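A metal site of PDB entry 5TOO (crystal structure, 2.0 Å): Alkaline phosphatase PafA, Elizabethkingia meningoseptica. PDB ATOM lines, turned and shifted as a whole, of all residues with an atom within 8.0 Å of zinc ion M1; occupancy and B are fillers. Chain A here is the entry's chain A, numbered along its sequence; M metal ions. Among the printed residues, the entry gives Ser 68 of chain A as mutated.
The backbone carbonyl oxygen (O) of Asp 27 lies within hydrogen-bond range of the backbone NH (N) of Asp 294 (3.4 Å). The backbone NH (N) of Asp 27 lies within hydrogen-bond range of the backbone carbonyl oxygen (O) of Leu 290 (3.1 Å). The backbone carbonyl oxygen (O) of Asp 27 is in hydrogen-bond range of the side-chain hydroxyl (OG1) of Thr 293. ND1 of His 342 sits close to ND1 of His 475 (3.3 Å). O of His 342 is in hydrogen-bond range of N of Met 29 (3.4 Å). The side-chain carboxylate (OD2) of Asp 341 sits close to a ring nitrogen (ND1) of His 72, at 3.4 Å. The side-chain carboxylate of Asp 341 lies within hydrogen-bond range of the backbone NH of Gln 28, at 3.2 Å. O of Asp 294 is in hydrogen-bond range of NE2 of Gln 28 (3.0 Å).
Asp 294 touches zinc ion M1. Four residues have an atom within 4 Å of zinc ion M1: Asp 27, Asp 294, Asp 341 and His 342. The nearest printed residue that does not touch zinc ion M1 is His 475 (4.2 Å).
Zinc ion M1 is bound by OD1 of Asp 27, NE2 of His 342 and OD2 of Asp 341. Zinc ion M1 has three donor atoms within binding distance.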
ATOM      1  N   VAL A  25      -8.873 -27.290  -9.377  1.00  0.00           N
ATOM      2  CA  VAL A  25      -9.230 -25.949  -9.800  1.00  0.00           C
ATOM      3  C   VAL A  25      -8.768 -24.993  -8.729  1.00  0.00           C
ATOM      4  O   VAL A  25      -9.174 -25.118  -7.567  1.00  0.00           O
ATOM      5  CB  VAL A  25     -10.731 -25.781 -10.067  1.00  0.00           C
ATOM      6  CG1 VAL A  25     -10.998 -24.366 -10.556  1.00  0.00           C
ATOM      7  CG2 VAL A  25     -11.229 -26.819 -11.079  1.00  0.00           C
ATOM      8  N   VAL A  26      -7.927 -24.049  -9.121  1.00  0.00           N
ATOM      9  CA  VAL A  26      -7.448 -23.000  -8.260  1.00  0.00           C
ATOM     10  C   VAL A  26      -8.292 -21.774  -8.553  1.00  0.00           C
ATOM     11  O   VAL A  26      -8.178 -21.149  -9.600  1.00  0.00           O
ATOM     12  CB  VAL A  26      -5.959 -22.709  -8.472  1.00  0.00           C
ATOM     13  CG1 VAL A  26      -5.493 -21.668  -7.431  1.00  0.00           C
ATOM     14  CG2 VAL A  26      -5.143 -24.014  -8.393  1.00  0.00           C
ATOM     15  N   ASP A  27      -9.188 -21.484  -7.630  1.00  0.00           N
ATOM     16  CA  ASP A  27     -10.202 -20.486  -7.849  1.00  0.00           C
ATOM     17  C   ASP A  27      -9.590 -19.092  -7.978  1.00  0.00           C
ATOM     18  O   ASP A  27      -8.733 -18.695  -7.184  1.00  0.00           O
ATOM     19  CB  ASP A  27     -11.211 -20.565  -6.696  1.00  0.00           C
ATOM     20  CG  ASP A  27     -12.560 -20.082  -7.077  1.00  0.00           C
ATOM     21  OD1 ASP A  27     -12.647 -18.988  -7.635  1.00  0.00           O
ATOM     22  OD2 ASP A  27     -13.548 -20.804  -6.787  1.00  0.00           O
ATOM     23  N   GLN A  28      -9.988 -18.349  -9.010  1.00  0.00           N
ATOM     24  CA  GLN A  28      -9.485 -16.997  -9.281  1.00  0.00           C
ATOM     25  C   GLN A  28      -8.011 -16.960  -9.697  1.00  0.00           C
ATOM     26  O   GLN A  28      -7.421 -15.857  -9.761  1.00  0.00           O
ATOM     27  CB  GLN A  28      -9.697 -16.080  -8.072  1.00  0.00           C
ATOM     28  CG  GLN A  28      -9.850 -14.615  -8.417  1.00  0.00           C
ATOM     29  CD  GLN A  28      -9.838 -13.674  -7.172  1.00  0.00           C
ATOM     30  OE1 GLN A  28      -8.904 -12.900  -6.984  1.00  0.00           O
ATOM     31  NE2 GLN A  28     -10.902 -13.740  -6.342  1.00  0.00           N
ATOM     32  N   MET A  29      -7.404 -18.097 -10.032  1.00  0.00           N
ATOM     33  CA  MET A  29      -6.006 -18.107 -10.458  1.00  0.00           C
ATOM     34  C   MET A  29      -5.870 -17.589 -11.891  1.00  0.00           C
ATOM     35  O   MET A  29      -6.137 -18.302 -12.860  1.00  0.00           O
ATOM     36  CB  MET A  29      -5.414 -19.495 -10.341  1.00  0.00           C
ATOM     37  CG  MET A  29      -3.960 -19.492 -10.691  1.00  0.00           C
ATOM     38  SD  MET A  29      -3.136 -21.041 -10.510  1.00  0.00           S
ATOM     39  CE  MET A  29      -1.580 -20.527 -11.206  1.00  0.00           C
ATOM     40  N   THR A  66     -17.939 -14.286 -16.215  1.00  0.00           N
ATOM     41  CA  THR A  66     -16.953 -15.186 -15.612  1.00  0.00           C
ATOM     42  C   THR A  66     -17.063 -15.156 -14.091  1.00  0.00           C
ATOM     43  O   THR A  66     -16.117 -14.804 -13.358  1.00  0.00           O
ATOM     44  CB  THR A  66     -15.548 -14.795 -16.069  1.00  0.00           C
ATOM     45  OG1 THR A  66     -15.373 -13.379 -15.928  1.00  0.00           O
ATOM     46  CG2 THR A  66     -15.328 -15.185 -17.587  1.00  0.00           C
ATOM     47  N   VAL A  67     -18.237 -15.551 -13.601  1.00  0.00           N
ATOM     48  CA  VAL A  67     -18.490 -15.564 -12.164  1.00  0.00           C
ATOM     49  C   VAL A  67     -18.321 -16.969 -11.588  1.00  0.00           C
ATOM     50  O   VAL A  67     -17.915 -17.908 -12.265  1.00  0.00           O
ATOM     51  CB  VAL A  67     -19.881 -15.014 -11.823  1.00  0.00           C
ATOM     52  CG1 VAL A  67     -19.984 -13.542 -12.255  1.00  0.00           C
ATOM     53  CG2 VAL A  67     -20.981 -15.838 -12.491  1.00  0.00           C
ATOM     54  N   SER A  68     -18.655 -17.073 -10.308  1.00  0.00           N
ATOM     55  CA  SER A  68     -18.614 -18.308  -9.568  1.00  0.00           C
ATOM     56  C   SER A  68     -19.592 -19.340 -10.123  1.00  0.00           C
ATOM     57  O   SER A  68     -20.556 -19.005 -10.813  1.00  0.00           O
ATOM     58  CB  SER A  68     -19.001 -18.020  -8.112  1.00  0.00           C
ATOM     59  OG  SER A  68     -18.408 -16.789  -7.717  1.00  0.00           O
ATOM     60  N   ALA A  69     -19.337 -20.597  -9.767  1.00  0.00           N
ATOM     61  CA  ALA A  69     -20.181 -21.743 -10.116  1.00  0.00           C
ATOM     62  C   ALA A  69     -20.078 -22.115 -11.598  1.00  0.00           C
ATOM     63  O   ALA A  69     -19.911 -23.286 -11.912  1.00  0.00           O
ATOM     64  CB  ALA A  69     -21.642 -21.486  -9.744  1.00  0.00           C
ATOM     65  N   ILE A  70     -20.141 -21.147 -12.503  1.00  0.00           N
ATOM     66  CA  ILE A  70     -20.144 -21.464 -13.934  1.00  0.00           C
ATOM     67  C   ILE A  70     -18.804 -22.076 -14.356  1.00  0.00           C
ATOM     68  O   ILE A  70     -18.759 -23.071 -15.090  1.00  0.00           O
ATOM     69  CB  ILE A  70     -20.453 -20.226 -14.790  1.00  0.00           C
ATOM     70  CG1 ILE A  70     -21.690 -19.461 -14.314  1.00  0.00           C
ATOM     71  CG2 ILE A  70     -20.631 -20.620 -16.251  1.00  0.00           C
ATOM     72  CD1 ILE A  70     -21.974 -18.143 -15.168  1.00  0.00           C
ATOM     73  N   GLY A  71     -17.699 -21.451 -13.944  1.00  0.00           N
ATOM     74  CA  GLY A  71     -16.396 -21.950 -14.344  1.00  0.00           C
ATOM     75  C   GLY A  71     -16.181 -23.392 -13.932  1.00  0.00           C
ATOM     76  O   GLY A  71     -15.689 -24.203 -14.709  1.00  0.00           O
ATOM     77  N   HIS A  72     -16.531 -23.717 -12.680  1.00  0.00           N
ATOM     78  CA  HIS A  72     -16.456 -25.082 -12.226  1.00  0.00           C
ATOM     79  C   HIS A  72     -17.364 -25.971 -13.062  1.00  0.00           C
ATOM     80  O   HIS A  72     -16.934 -27.009 -13.577  1.00  0.00           O
ATOM     81  CB  HIS A  72     -16.817 -25.158 -10.722  1.00  0.00           C
ATOM     82  CG  HIS A  72     -15.789 -24.499  -9.857  1.00  0.00           C
ATOM     83  ND1 HIS A  72     -15.932 -23.234  -9.338  1.00  0.00           N
ATOM     84  CD2 HIS A  72     -14.562 -24.932  -9.476  1.00  0.00           C
ATOM     85  CE1 HIS A  72     -14.842 -22.912  -8.661  1.00  0.00           C
ATOM     86  NE2 HIS A  72     -13.996 -23.930  -8.727  1.00  0.00           N
ATOM     87  N   ALA A 154     -18.397 -25.515  -5.660  1.00  0.00           N
ATOM     88  CA  ALA A 154     -17.145 -25.979  -6.230  1.00  0.00           C
ATOM     89  C   ALA A 154     -16.829 -27.426  -5.873  1.00  0.00           C
ATOM     90  O   ALA A 154     -15.923 -28.019  -6.479  1.00  0.00           O
ATOM     91  CB  ALA A 154     -16.022 -25.033  -5.758  1.00  0.00           C
ATOM     92  N   ASN A 289     -11.312 -28.191  -5.510  1.00  0.00           N
ATOM     93  CA  ASN A 289     -11.270 -26.756  -5.736  1.00  0.00           C
ATOM     94  C   ASN A 289     -10.530 -26.135  -4.569  1.00  0.00           C
ATOM     95  O   ASN A 289     -10.829 -26.431  -3.411  1.00  0.00           O
ATOM     96  CB  ASN A 289     -12.672 -26.154  -5.844  1.00  0.00           C
ATOM     97  CG  ASN A 289     -12.660 -24.618  -5.848  1.00  0.00           C
ATOM     98  OD1 ASN A 289     -12.075 -24.008  -6.730  1.00  0.00           O
ATOM     99  ND2 ASN A 289     -13.291 -24.003  -4.861  1.00  0.00           N
ATOM    100  N   LEU A 290      -9.545 -25.303  -4.876  1.00  0.00           N
ATOM    101  CA  LEU A 290      -8.786 -24.549  -3.883  1.00  0.00           C
ATOM    102  C   LEU A 290      -9.429 -23.173  -3.803  1.00  0.00           C
ATOM    103  O   LEU A 290      -9.095 -22.285  -4.594  1.00  0.00           O
ATOM    104  CB  LEU A 290      -7.306 -24.462  -4.262  1.00  0.00           C
ATOM    105  CG  LEU A 290      -6.409 -25.711  -4.171  1.00  0.00           C
ATOM    106  CD1 LEU A 290      -6.608 -26.485  -2.895  1.00  0.00           C
ATOM    107  CD2 LEU A 290      -6.548 -26.691  -5.287  1.00  0.00           C
ATOM    108  N   ALA A 291     -10.321 -22.974  -2.841  1.00  0.00           N
ATOM    109  CA  ALA A 291     -11.145 -21.763  -2.822  1.00  0.00           C
ATOM    110  C   ALA A 291     -10.441 -20.546  -2.240  1.00  0.00           C
ATOM    111  O   ALA A 291     -10.882 -19.427  -2.502  1.00  0.00           O
ATOM    112  CB  ALA A 291     -12.424 -22.011  -2.027  1.00  0.00           C
ATOM    113  N   THR A 293      -7.632 -19.001  -2.679  1.00  0.00           N
ATOM    114  CA  THR A 293      -7.093 -18.000  -3.626  1.00  0.00           C
ATOM    115  C   THR A 293      -8.151 -16.974  -4.006  1.00  0.00           C
ATOM    116  O   THR A 293      -7.848 -15.800  -4.249  1.00  0.00           O
ATOM    117  CB  THR A 293      -6.551 -18.696  -4.880  1.00  0.00           C
ATOM    118  OG1 THR A 293      -7.314 -19.904  -5.141  1.00  0.00           O
ATOM    119  CG2 THR A 293      -5.114 -19.086  -4.684  1.00  0.00           C
ATOM    120  N   ASP A 294      -9.409 -17.396  -4.068  1.00  0.00           N
ATOM    121  CA  ASP A 294     -10.486 -16.480  -4.422  1.00  0.00           C
ATOM    122  C   ASP A 294     -10.835 -15.557  -3.260  1.00  0.00           C
ATOM    123  O   ASP A 294     -10.823 -14.327  -3.413  1.00  0.00           O
ATOM    124  CB  ASP A 294     -11.694 -17.296  -4.873  1.00  0.00           C
ATOM    125  CG  ASP A 294     -12.861 -16.452  -5.250  1.00  0.00           C
ATOM    126  OD1 ASP A 294     -12.874 -15.880  -6.372  1.00  0.00           O
ATOM    127  OD2 ASP A 294     -13.775 -16.383  -4.427  1.00  0.00           O
ATOM    128  N   TYR A 295     -11.151 -16.134  -2.107  1.00  0.00           N
ATOM    129  CA  TYR A 295     -11.408 -15.330  -0.914  1.00  0.00           C
ATOM    130  C   TYR A 295     -10.316 -14.293  -0.676  1.00  0.00           C
ATOM    131  O   TYR A 295     -10.597 -13.114  -0.508  1.00  0.00           O
ATOM    132  CB  TYR A 295     -11.530 -16.246   0.299  1.00  0.00           C
ATOM    133  CG  TYR A 295     -12.823 -16.963   0.299  1.00  0.00           C
ATOM    134  CD1 TYR A 295     -13.972 -16.344   0.763  1.00  0.00           C
ATOM    135  CD2 TYR A 295     -12.902 -18.268  -0.166  1.00  0.00           C
ATOM    136  CE1 TYR A 295     -15.168 -17.016   0.785  1.00  0.00           C
ATOM    137  CE2 TYR A 295     -14.080 -18.949  -0.165  1.00  0.00           C
ATOM    138  CZ  TYR A 295     -15.223 -18.320   0.290  1.00  0.00           C
ATOM    139  OH  TYR A 295     -16.412 -19.018   0.299  1.00  0.00           O
ATOM    140  N   HIS A 298     -10.390 -11.835  -3.468  1.00  0.00           N
ATOM    141  CA  HIS A 298     -11.504 -10.895  -3.377  1.00  0.00           C
ATOM    142  C   HIS A 298     -11.211  -9.791  -2.379  1.00  0.00           C
ATOM    143  O   HIS A 298     -11.668  -8.661  -2.570  1.00  0.00           O
ATOM    144  CB  HIS A 298     -12.794 -11.617  -2.984  1.00  0.00           C
ATOM    145  CG  HIS A 298     -13.542 -12.172  -4.164  1.00  0.00           C
ATOM    146  ND1 HIS A 298     -14.110 -11.363  -5.117  1.00  0.00           N
ATOM    147  CD2 HIS A 298     -13.783 -13.439  -4.543  1.00  0.00           C
ATOM    148  CE1 HIS A 298     -14.684 -12.122  -6.039  1.00  0.00           C
ATOM    149  NE2 HIS A 298     -14.491 -13.383  -5.717  1.00  0.00           N
ATOM    150  N   ALA A 340      -8.247 -23.042 -13.658  1.00  0.00           N
ATOM    151  CA  ALA A 340      -8.932 -22.048 -12.860  1.00  0.00           C
ATOM    152  C   ALA A 340     -10.314 -21.867 -13.442  1.00  0.00           C
ATOM    153  O   ALA A 340     -10.535 -22.127 -14.616  1.00  0.00           O
ATOM    154  CB  ALA A 340      -8.217 -20.700 -12.857  1.00  0.00           C
ATOM    155  N   ASP A 341     -11.238 -21.368 -12.617  1.00  0.00           N
ATOM    156  CA  ASP A 341     -12.613 -21.122 -13.038  1.00  0.00           C
ATOM    157  C   ASP A 341     -12.798 -19.688 -13.510  1.00  0.00           C
ATOM    158  O   ASP A 341     -13.870 -19.342 -14.014  1.00  0.00           O
ATOM    159  CB  ASP A 341     -13.561 -21.449 -11.891  1.00  0.00           C
ATOM    160  CG  ASP A 341     -13.361 -20.545 -10.680  1.00  0.00           C
ATOM    161  OD1 ASP A 341     -12.233 -20.071 -10.447  1.00  0.00           O
ATOM    162  OD2 ASP A 341     -14.358 -20.302  -9.971  1.00  0.00           O
ATOM    163  N   HIS A 342     -11.760 -18.875 -13.372  1.00  0.00           N
ATOM    164  CA  HIS A 342     -11.713 -17.481 -13.806  1.00  0.00           C
ATOM    165  C   HIS A 342     -10.447 -16.843 -13.272  1.00  0.00           C
ATOM    166  O   HIS A 342      -9.779 -17.406 -12.395  1.00  0.00           O
ATOM    167  CB  HIS A 342     -12.924 -16.674 -13.323  1.00  0.00           C
ATOM    168  CG  HIS A 342     -13.118 -16.707 -11.834  1.00  0.00           C
ATOM    169  ND1 HIS A 342     -12.411 -15.900 -10.979  1.00  0.00           N
ATOM    170  CD2 HIS A 342     -13.926 -17.472 -11.055  1.00  0.00           C
ATOM    171  CE1 HIS A 342     -12.778 -16.156  -9.730  1.00  0.00           C
ATOM    172  NE2 HIS A 342     -13.702 -17.093  -9.745  1.00  0.00           N
ATOM    173  N   GLY A 343     -10.108 -15.680 -13.808  1.00  0.00           N
ATOM    174  CA  GLY A 343      -9.013 -14.859 -13.333  1.00  0.00           C
ATOM    175  C   GLY A 343      -9.546 -13.789 -12.396  1.00  0.00           C
ATOM    176  O   GLY A 343     -10.445 -14.046 -11.580  1.00  0.00           O
ATOM    177  N   HIS A 475     -14.334 -10.567 -10.411  1.00  0.00           N
ATOM    178  CA  HIS A 475     -14.250 -11.190 -11.723  1.00  0.00           C
ATOM    179  C   HIS A 475     -15.653 -11.259 -12.285  1.00  0.00           C
ATOM    180  O   HIS A 475     -16.586 -11.589 -11.551  1.00  0.00           O
ATOM    181  CB  HIS A 475     -13.688 -12.608 -11.601  1.00  0.00           C
ATOM    182  CG  HIS A 475     -14.321 -13.401 -10.492  1.00  0.00           C
ATOM    183  ND1 HIS A 475     -15.324 -14.329 -10.713  1.00  0.00           N
ATOM    184  CD2 HIS A 475     -14.104 -13.386  -9.156  1.00  0.00           C
ATOM    185  CE1 HIS A 475     -15.673 -14.864  -9.557  1.00  0.00           C
ATOM    186  NE2 HIS A 475     -14.959 -14.301  -8.600  1.00  0.00           N
HETATM  187 ZN    ZN M   1     -14.346 -18.684  -8.613  1.00  0.00          ZN
HETATM  188 ZN    ZN M   2     -14.814 -15.141  -6.645  1.00  0.00          ZN
